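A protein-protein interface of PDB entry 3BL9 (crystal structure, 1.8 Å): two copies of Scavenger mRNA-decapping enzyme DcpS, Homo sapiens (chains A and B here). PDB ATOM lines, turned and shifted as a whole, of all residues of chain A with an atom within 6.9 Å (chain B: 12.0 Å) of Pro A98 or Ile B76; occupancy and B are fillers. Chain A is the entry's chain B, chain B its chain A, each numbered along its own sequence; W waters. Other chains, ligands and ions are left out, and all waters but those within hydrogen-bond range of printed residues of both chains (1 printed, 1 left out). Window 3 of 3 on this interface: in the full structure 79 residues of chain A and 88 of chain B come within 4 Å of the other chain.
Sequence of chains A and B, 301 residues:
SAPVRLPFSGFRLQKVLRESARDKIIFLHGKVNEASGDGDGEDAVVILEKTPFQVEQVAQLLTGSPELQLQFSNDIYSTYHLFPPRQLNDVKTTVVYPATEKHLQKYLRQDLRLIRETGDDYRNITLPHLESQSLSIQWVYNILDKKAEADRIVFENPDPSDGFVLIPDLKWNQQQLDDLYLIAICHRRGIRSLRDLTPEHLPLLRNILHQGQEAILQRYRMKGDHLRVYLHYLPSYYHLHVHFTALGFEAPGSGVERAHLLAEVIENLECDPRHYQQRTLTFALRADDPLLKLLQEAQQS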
ATOM      1  N   PRO A   7     -27.196  -6.041 -19.914  1.00  0.00           N
ATOM      2  CA  PRO A   7     -27.572  -7.336 -19.356  1.00  0.00           C
ATOM      3  C   PRO A   7     -26.650  -7.806 -18.234  1.00  0.00           C
ATOM      4  O   PRO A   7     -26.522  -9.021 -18.021  1.00  0.00           O
ATOM      5  CB  PRO A   7     -27.475  -8.262 -20.571  1.00  0.00           C
ATOM      6  CG  PRO A   7     -26.400  -7.680 -21.386  1.00  0.00           C
ATOM      7  CD  PRO A   7     -26.425  -6.198 -21.163  1.00  0.00           C
ATOM      8  N   GLU A  42     -16.524 -12.008 -14.431  1.00  0.00           N
ATOM      9  CA  GLU A  42     -17.109 -12.330 -15.735  1.00  0.00           C
ATOM     10  C   GLU A  42     -16.724 -11.277 -16.795  1.00  0.00           C
ATOM     11  O   GLU A  42     -16.476 -10.105 -16.482  1.00  0.00           O
ATOM     12  CB  GLU A  42     -18.635 -12.467 -15.648  1.00  0.00           C
ATOM     13  N   ASP A  43     -16.699 -11.740 -18.035  1.00  0.00           N
ATOM     14  CA  ASP A  43     -16.214 -10.982 -19.181  1.00  0.00           C
ATOM     15  C   ASP A  43     -17.367 -10.620 -20.092  1.00  0.00           C
ATOM     16  O   ASP A  43     -18.228 -11.470 -20.392  1.00  0.00           O
ATOM     17  CB  ASP A  43     -15.243 -11.833 -20.002  1.00  0.00           C
ATOM     18  CG  ASP A  43     -13.923 -12.081 -19.300  1.00  0.00           C
ATOM     19  OD1 ASP A  43     -13.323 -11.110 -18.791  1.00  0.00           O
ATOM     20  OD2 ASP A  43     -13.471 -13.254 -19.303  1.00  0.00           O
ATOM     21  N   ALA A  44     -17.348  -9.375 -20.568  1.00  0.00           N
ATOM     22  CA  ALA A  44     -18.274  -8.908 -21.578  1.00  0.00           C
ATOM     23  C   ALA A  44     -17.461  -8.234 -22.696  1.00  0.00           C
ATOM     24  O   ALA A  44     -16.438  -7.586 -22.420  1.00  0.00           O
ATOM     25  CB  ALA A  44     -19.254  -7.910 -20.972  1.00  0.00           C
ATOM     26  N   VAL A  45     -17.907  -8.414 -23.934  1.00  0.00           N
ATOM     27  CA  VAL A  45     -17.482  -7.547 -25.036  1.00  0.00           C
ATOM     28  C   VAL A  45     -18.621  -6.579 -25.369  1.00  0.00           C
ATOM     29  O   VAL A  45     -19.758  -6.992 -25.602  1.00  0.00           O
ATOM     30  CB  VAL A  45     -17.097  -8.340 -26.292  1.00  0.00           C
ATOM     31  CG1 VAL A  45     -16.729  -7.385 -27.446  1.00  0.00           C
ATOM     32  CG2 VAL A  45     -15.928  -9.312 -25.995  1.00  0.00           C
ATOM     33  N   VAL A  95     -23.677  -6.129 -27.357  1.00  0.00           N
ATOM     34  CA  VAL A  95     -23.132  -6.697 -26.135  1.00  0.00           C
ATOM     35  C   VAL A  95     -23.049  -8.215 -26.307  1.00  0.00           C
ATOM     36  O   VAL A  95     -24.020  -8.855 -26.744  1.00  0.00           O
ATOM     37  CB  VAL A  95     -23.999  -6.342 -24.899  1.00  0.00           C
ATOM     38  CG1 VAL A  95     -23.360  -6.857 -23.651  1.00  0.00           C
ATOM     39  CG2 VAL A  95     -24.212  -4.848 -24.797  1.00  0.00           C
ATOM     40  N   VAL A  96     -21.878  -8.771 -25.997  1.00  0.00           N
ATOM     41  CA  VAL A  96     -21.685 -10.214 -25.938  1.00  0.00           C
ATOM     42  C   VAL A  96     -21.433 -10.513 -24.468  1.00  0.00           C
ATOM     43  O   VAL A  96     -20.441 -10.041 -23.890  1.00  0.00           O
ATOM     44  CB  VAL A  96     -20.492 -10.696 -26.804  1.00  0.00           C
ATOM     45  CG1 VAL A  96     -20.412 -12.237 -26.822  1.00  0.00           C
ATOM     46  CG2 VAL A  96     -20.606 -10.145 -28.216  1.00  0.00           C
ATOM     47  N   TYR A  97     -22.356 -11.246 -23.838  1.00  0.00           N
ATOM     48  CA  TYR A  97     -22.203 -11.560 -22.423  1.00  0.00           C
ATOM     49  C   TYR A  97     -22.897 -12.878 -22.042  1.00  0.00           C
ATOM     50  O   TYR A  97     -24.084 -13.035 -22.312  1.00  0.00           O
ATOM     51  CB  TYR A  97     -22.733 -10.424 -21.538  1.00  0.00           C
ATOM     52  CG  TYR A  97     -22.741 -10.795 -20.066  1.00  0.00           C
ATOM     53  CD1 TYR A  97     -21.555 -11.067 -19.389  1.00  0.00           C
ATOM     54  CD2 TYR A  97     -23.933 -10.930 -19.364  1.00  0.00           C
ATOM     55  CE1 TYR A  97     -21.551 -11.431 -18.038  1.00  0.00           C
ATOM     56  CE2 TYR A  97     -23.939 -11.291 -18.019  1.00  0.00           C
ATOM     57  CZ  TYR A  97     -22.755 -11.552 -17.368  1.00  0.00           C
ATOM     58  OH  TYR A  97     -22.781 -11.916 -16.038  1.00  0.00           O
ATOM     59  N   PRO A  98     -22.149 -13.818 -21.430  1.00  0.00           N
ATOM     60  CA  PRO A  98     -20.725 -13.787 -21.131  1.00  0.00           C
ATOM     61  C   PRO A  98     -19.886 -14.023 -22.367  1.00  0.00           C
ATOM     62  O   PRO A  98     -20.289 -14.783 -23.259  1.00  0.00           O
ATOM     63  CB  PRO A  98     -20.530 -14.956 -20.143  1.00  0.00           C
ATOM     64  CG  PRO A  98     -21.870 -15.381 -19.762  1.00  0.00           C
ATOM     65  CD  PRO A  98     -22.734 -15.071 -20.942  1.00  0.00           C
ATOM     66  N   ALA A  99     -18.728 -13.366 -22.415  1.00  0.00           N
ATOM     67  CA  ALA A  99     -17.785 -13.557 -23.502  1.00  0.00           C
ATOM     68  C   ALA A  99     -16.812 -14.659 -23.111  1.00  0.00           C
ATOM     69  O   ALA A  99     -16.236 -14.634 -22.025  1.00  0.00           O
ATOM     70  CB  ALA A  99     -17.035 -12.265 -23.789  1.00  0.00           C
ATOM     71  N   THR A 100     -16.643 -15.620 -24.012  1.00  0.00           N
ATOM     72  CA  THR A 100     -15.675 -16.703 -23.853  1.00  0.00           C
ATOM     73  C   THR A 100     -14.309 -16.244 -24.367  1.00  0.00           C
ATOM     74  O   THR A 100     -14.206 -15.212 -25.038  1.00  0.00           O
ATOM     75  CB  THR A 100     -16.110 -17.924 -24.657  1.00  0.00           C
ATOM     76  OG1 THR A 100     -16.085 -17.609 -26.054  1.00  0.00           O
ATOM     77  CG2 THR A 100     -17.527 -18.350 -24.270  1.00  0.00           C
ATOM     78  N   HIS A 103     -14.394 -15.498 -28.060  1.00  0.00           N
ATOM     79  CA  HIS A 103     -14.891 -14.165 -28.433  1.00  0.00           C
ATOM     80  C   HIS A 103     -13.768 -13.145 -28.321  1.00  0.00           C
ATOM     81  O   HIS A 103     -13.504 -12.401 -29.256  1.00  0.00           O
ATOM     82  CB  HIS A 103     -16.061 -13.724 -27.549  1.00  0.00           C
ATOM     83  CG  HIS A 103     -17.341 -14.435 -27.847  1.00  0.00           C
ATOM     84  ND1 HIS A 103     -17.910 -15.342 -26.976  1.00  0.00           N
ATOM     85  CD2 HIS A 103     -18.155 -14.388 -28.929  1.00  0.00           C
ATOM     86  CE1 HIS A 103     -19.024 -15.816 -27.507  1.00  0.00           C
ATOM     87  NE2 HIS A 103     -19.196 -15.251 -28.690  1.00  0.00           N
ATOM     88  N   LEU B  70     -33.428  -1.317 -26.435  1.00  0.00           N
ATOM     89  CA  LEU B  70     -33.089  -2.671 -26.895  1.00  0.00           C
ATOM     90  C   LEU B  70     -33.662  -2.912 -28.283  1.00  0.00           C
ATOM     91  O   LEU B  70     -34.877  -2.847 -28.463  1.00  0.00           O
ATOM     92  CB  LEU B  70     -33.626  -3.724 -25.918  1.00  0.00           C
ATOM     93  CG  LEU B  70     -33.358  -5.205 -26.216  1.00  0.00           C
ATOM     94  CD1 LEU B  70     -31.873  -5.523 -26.063  1.00  0.00           C
ATOM     95  CD2 LEU B  70     -34.199  -6.099 -25.295  1.00  0.00           C
ATOM     96  N   PHE B  72     -32.650  -5.773 -30.396  1.00  0.00           N
ATOM     97  CA  PHE B  72     -32.925  -7.212 -30.357  1.00  0.00           C
ATOM     98  C   PHE B  72     -31.986  -7.961 -29.438  1.00  0.00           C
ATOM     99  O   PHE B  72     -30.961  -7.442 -29.019  1.00  0.00           O
ATOM    100  CB  PHE B  72     -32.956  -7.835 -31.770  1.00  0.00           C
ATOM    101  CG  PHE B  72     -31.692  -7.665 -32.563  1.00  0.00           C
ATOM    102  CD1 PHE B  72     -30.632  -8.564 -32.410  1.00  0.00           C
ATOM    103  CD2 PHE B  72     -31.583  -6.646 -33.513  1.00  0.00           C
ATOM    104  CE1 PHE B  72     -29.457  -8.423 -33.165  1.00  0.00           C
ATOM    105  CE2 PHE B  72     -30.417  -6.492 -34.277  1.00  0.00           C
ATOM    106  CZ  PHE B  72     -29.350  -7.379 -34.102  1.00  0.00           C
ATOM    107  N   SER B  73     -32.374  -9.184 -29.107  1.00  0.00           N
ATOM    108  CA  SER B  73     -31.672  -9.977 -28.119  1.00  0.00           C
ATOM    109  C   SER B  73     -31.808 -11.476 -28.436  1.00  0.00           C
ATOM    110  O   SER B  73     -32.872 -11.929 -28.870  1.00  0.00           O
ATOM    111  CB  SER B  73     -32.244  -9.656 -26.735  1.00  0.00           C
ATOM    112  OG  SER B  73     -31.849 -10.603 -25.765  1.00  0.00           O
ATOM    113  N   ASN B  74     -30.723 -12.219 -28.229  1.00  0.00           N
ATOM    114  CA  ASN B  74     -30.712 -13.679 -28.395  1.00  0.00           C
ATOM    115  C   ASN B  74     -29.590 -14.303 -27.582  1.00  0.00           C
ATOM    116  O   ASN B  74     -28.410 -14.243 -27.958  1.00  0.00           O
ATOM    117  CB  ASN B  74     -30.617 -14.095 -29.869  1.00  0.00           C
ATOM    118  CG  ASN B  74     -29.707 -13.188 -30.682  1.00  0.00           C
ATOM    119  OD1 ASN B  74     -30.123 -12.107 -31.147  1.00  0.00           O
ATOM    120  ND2 ASN B  74     -28.463 -13.630 -30.881  1.00  0.00           N
ATOM    121  N   ASP B  75     -29.994 -14.902 -26.464  1.00  0.00           N
ATOM    122  CA  ASP B  75     -29.104 -15.426 -25.420  1.00  0.00           C
ATOM    123  C   ASP B  75     -27.950 -14.479 -25.042  1.00  0.00           C
ATOM    124  O   ASP B  75     -28.204 -13.436 -24.437  1.00  0.00           O
ATOM    125  CB  ASP B  75     -28.616 -16.839 -25.766  1.00  0.00           C
ATOM    126  CG  ASP B  75     -28.097 -17.592 -24.536  1.00  0.00           C
ATOM    127  OD1 ASP B  75     -27.971 -16.968 -23.457  1.00  0.00           O
ATOM    128  OD2 ASP B  75     -27.820 -18.808 -24.650  1.00  0.00           O
ATOM    129  N   ILE B  76     -26.707 -14.821 -25.390  1.00  0.00           N
ATOM    130  CA  ILE B  76     -25.557 -14.014 -24.962  1.00  0.00           C
ATOM    131  C   ILE B  76     -25.368 -12.735 -25.786  1.00  0.00           C
ATOM    132  O   ILE B  76     -24.577 -11.878 -25.402  1.00  0.00           O
ATOM    133  CB  ILE B  76     -24.207 -14.799 -24.971  1.00  0.00           C
ATOM    134  CG1 ILE B  76     -23.737 -15.093 -26.406  1.00  0.00           C
ATOM    135  CG2 ILE B  76     -24.305 -16.079 -24.115  1.00  0.00           C
ATOM    136  CD1 ILE B  76     -22.360 -15.720 -26.457  1.00  0.00           C
ATOM    137  N   TYR B  77     -26.091 -12.620 -26.900  1.00  0.00           N
ATOM    138  CA  TYR B  77     -26.006 -11.474 -27.804  1.00  0.00           C
ATOM    139  C   TYR B  77     -27.185 -10.526 -27.640  1.00  0.00           C
ATOM    140  O   TYR B  77     -28.345 -10.958 -27.675  1.00  0.00           O
ATOM    141  CB  TYR B  77     -25.995 -11.967 -29.257  1.00  0.00           C
ATOM    142  CG  TYR B  77     -24.900 -12.971 -29.547  1.00  0.00           C
ATOM    143  CD1 TYR B  77     -25.146 -14.346 -29.499  1.00  0.00           C
ATOM    144  CD2 TYR B  77     -23.611 -12.547 -29.862  1.00  0.00           C
ATOM    145  CE1 TYR B  77     -24.125 -15.275 -29.767  1.00  0.00           C
ATOM    146  CE2 TYR B  77     -22.593 -13.464 -30.125  1.00  0.00           C
ATOM    147  CZ  TYR B  77     -22.856 -14.822 -30.083  1.00  0.00           C
ATOM    148  OH  TYR B  77     -21.830 -15.721 -30.347  1.00  0.00           O
ATOM    149  N   SER B  78     -26.901  -9.234 -27.483  1.00  0.00           N
ATOM    150  CA  SER B  78     -27.958  -8.223 -27.584  1.00  0.00           C
ATOM    151  C   SER B  78     -27.467  -6.956 -28.293  1.00  0.00           C
ATOM    152  O   SER B  78     -26.290  -6.606 -28.204  1.00  0.00           O
ATOM    153  CB  SER B  78     -28.515  -7.888 -26.218  1.00  0.00           C
ATOM    154  OG  SER B  78     -27.478  -7.591 -25.330  1.00  0.00           O
ATOM    155  N   THR B  79     -28.386  -6.298 -28.990  1.00  0.00           N
ATOM    156  CA  THR B  79     -28.094  -5.075 -29.732  1.00  0.00           C
ATOM    157  C   THR B  79     -28.971  -3.946 -29.199  1.00  0.00           C
ATOM    158  O   THR B  79     -30.170  -4.139 -28.963  1.00  0.00           O
ATOM    159  CB  THR B  79     -28.327  -5.291 -31.236  1.00  0.00           C
ATOM    160  OG1 THR B  79     -27.442  -6.323 -31.699  1.00  0.00           O
ATOM    161  CG2 THR B  79     -28.081  -4.002 -32.043  1.00  0.00           C
ATOM    162  N   TYR B  80     -28.367  -2.773 -29.015  1.00  0.00           N
ATOM    163  CA  TYR B  80     -29.077  -1.606 -28.508  1.00  0.00           C
ATOM    164  C   TYR B  80     -28.847  -0.369 -29.352  1.00  0.00           C
ATOM    165  O   TYR B  80     -27.938  -0.327 -30.180  1.00  0.00           O
ATOM    166  CB  TYR B  80     -28.624  -1.245 -27.102  1.00  0.00           C
ATOM    167  CG  TYR B  80     -28.751  -2.303 -26.040  1.00  0.00           C
ATOM    168  CD1 TYR B  80     -27.748  -3.242 -25.852  1.00  0.00           C
ATOM    169  CD2 TYR B  80     -29.838  -2.311 -25.154  1.00  0.00           C
ATOM    170  CE1 TYR B  80     -27.827  -4.194 -24.852  1.00  0.00           C
ATOM    171  CE2 TYR B  80     -29.926  -3.272 -24.142  1.00  0.00           C
ATOM    172  CZ  TYR B  80     -28.912  -4.202 -23.997  1.00  0.00           C
ATOM    173  OH  TYR B  80     -28.966  -5.166 -23.000  1.00  0.00           O
HETATM  174  O   HOH W   1     -25.849  -9.443 -24.269  1.00  0.00           O
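The backbone carbonyl oxygen (O) of Ile B76 is in hydrogen-bond range of the backbone NH (N) of Tyr A97, 2.8 Å away. A ring nitrogen (NE2) of His A103 lies within hydrogen-bond range of the side-chain hydroxyl (OH) of Tyr B77 (3.1 Å). The backbone carbonyl oxygen of Ser B78 sits at hydrogen-bond distance from the backbone NH of Val A95, 2.8 Å away. The backbone carbonyl oxygen of Val A95 sits close to the backbone carbonyl oxygen of Ile B76 (3.4 Å).
The backbone NH (N) of Val A96 sits at hydrogen-bond distance from the backbone carbonyl oxygen (O) of Val A45 (2.8 Å). ND1 of His A103 is in hydrogen-bond range of OG1 of Thr A100.
Pro A7 touches Tyr B80. Val A95 touches Tyr B77 (O to CA, 3.5 Å). Tyr B80 touches Val A95. Ile B76 touches Val A96 (O to CA, 3.4 Å). Pro A98 touches Ile B76 (CD to CG2, 3.7 Å). Ile B76 touches His A103 (CD1 to CE1, 3.5 Å).
Of chain B, only Ile B76 (3.7 Å) comes within 4 Å of Pro A98. Ile B76 touches five residues of chain A. No residue of chain B comes within 4 Å of Glu A42. Ala A44 touches none of the printed residues of chain B. Val A95 touches just these residues of chain B: Ile B76, Tyr B77, Ser B78 and Tyr B80. Of chain B, only Ile B76 comes within 4 Å of Tyr A97. Ala A99 touches none of the printed residues of chain B. No residue of chain B comes within 4 Å of Thr A100. Printed residues of chain B within 4 Å of His A103: Ile B76 and Tyr B77. Of the printed residues of chain A, Tyr B77 touches Val A95 (3.5 Å) and His A103 (3.1 Å). Ser B73 touches none of the printed residues of chain A. The nearest residue of chain A that does not touch Ile B76 is Ala A99 (5.9 Å). The nearest printed residue of chain B that does not touch His A103 is Asn B74 (9.3 Å).
Printed residues of chain A that touch a printed residue of chain B: Pro A7, Val A95, Val A96, Tyr A97, Pro A98 and His A103. Hydrophobic or aromatic side chains of chain B within 4 Å of the printed part of chain A: Ile B76, Tyr B77 and Tyr B80. Among the printed residues, no Asp or Glu carboxylate lies within 4 Å of a Lys or Arg side-chain nitrogen of the other chain.
No position is printed for both chains.
Water W1 lies within hydrogen-bond range of the side-chain hydroxyl (OG) of Ser B78 (2.7 Å), the backbone carbonyl oxygen (O) of Ile B76 (3.0 Å) and the backbone carbonyl oxygen (O) of Val A95 (3.1 Å).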
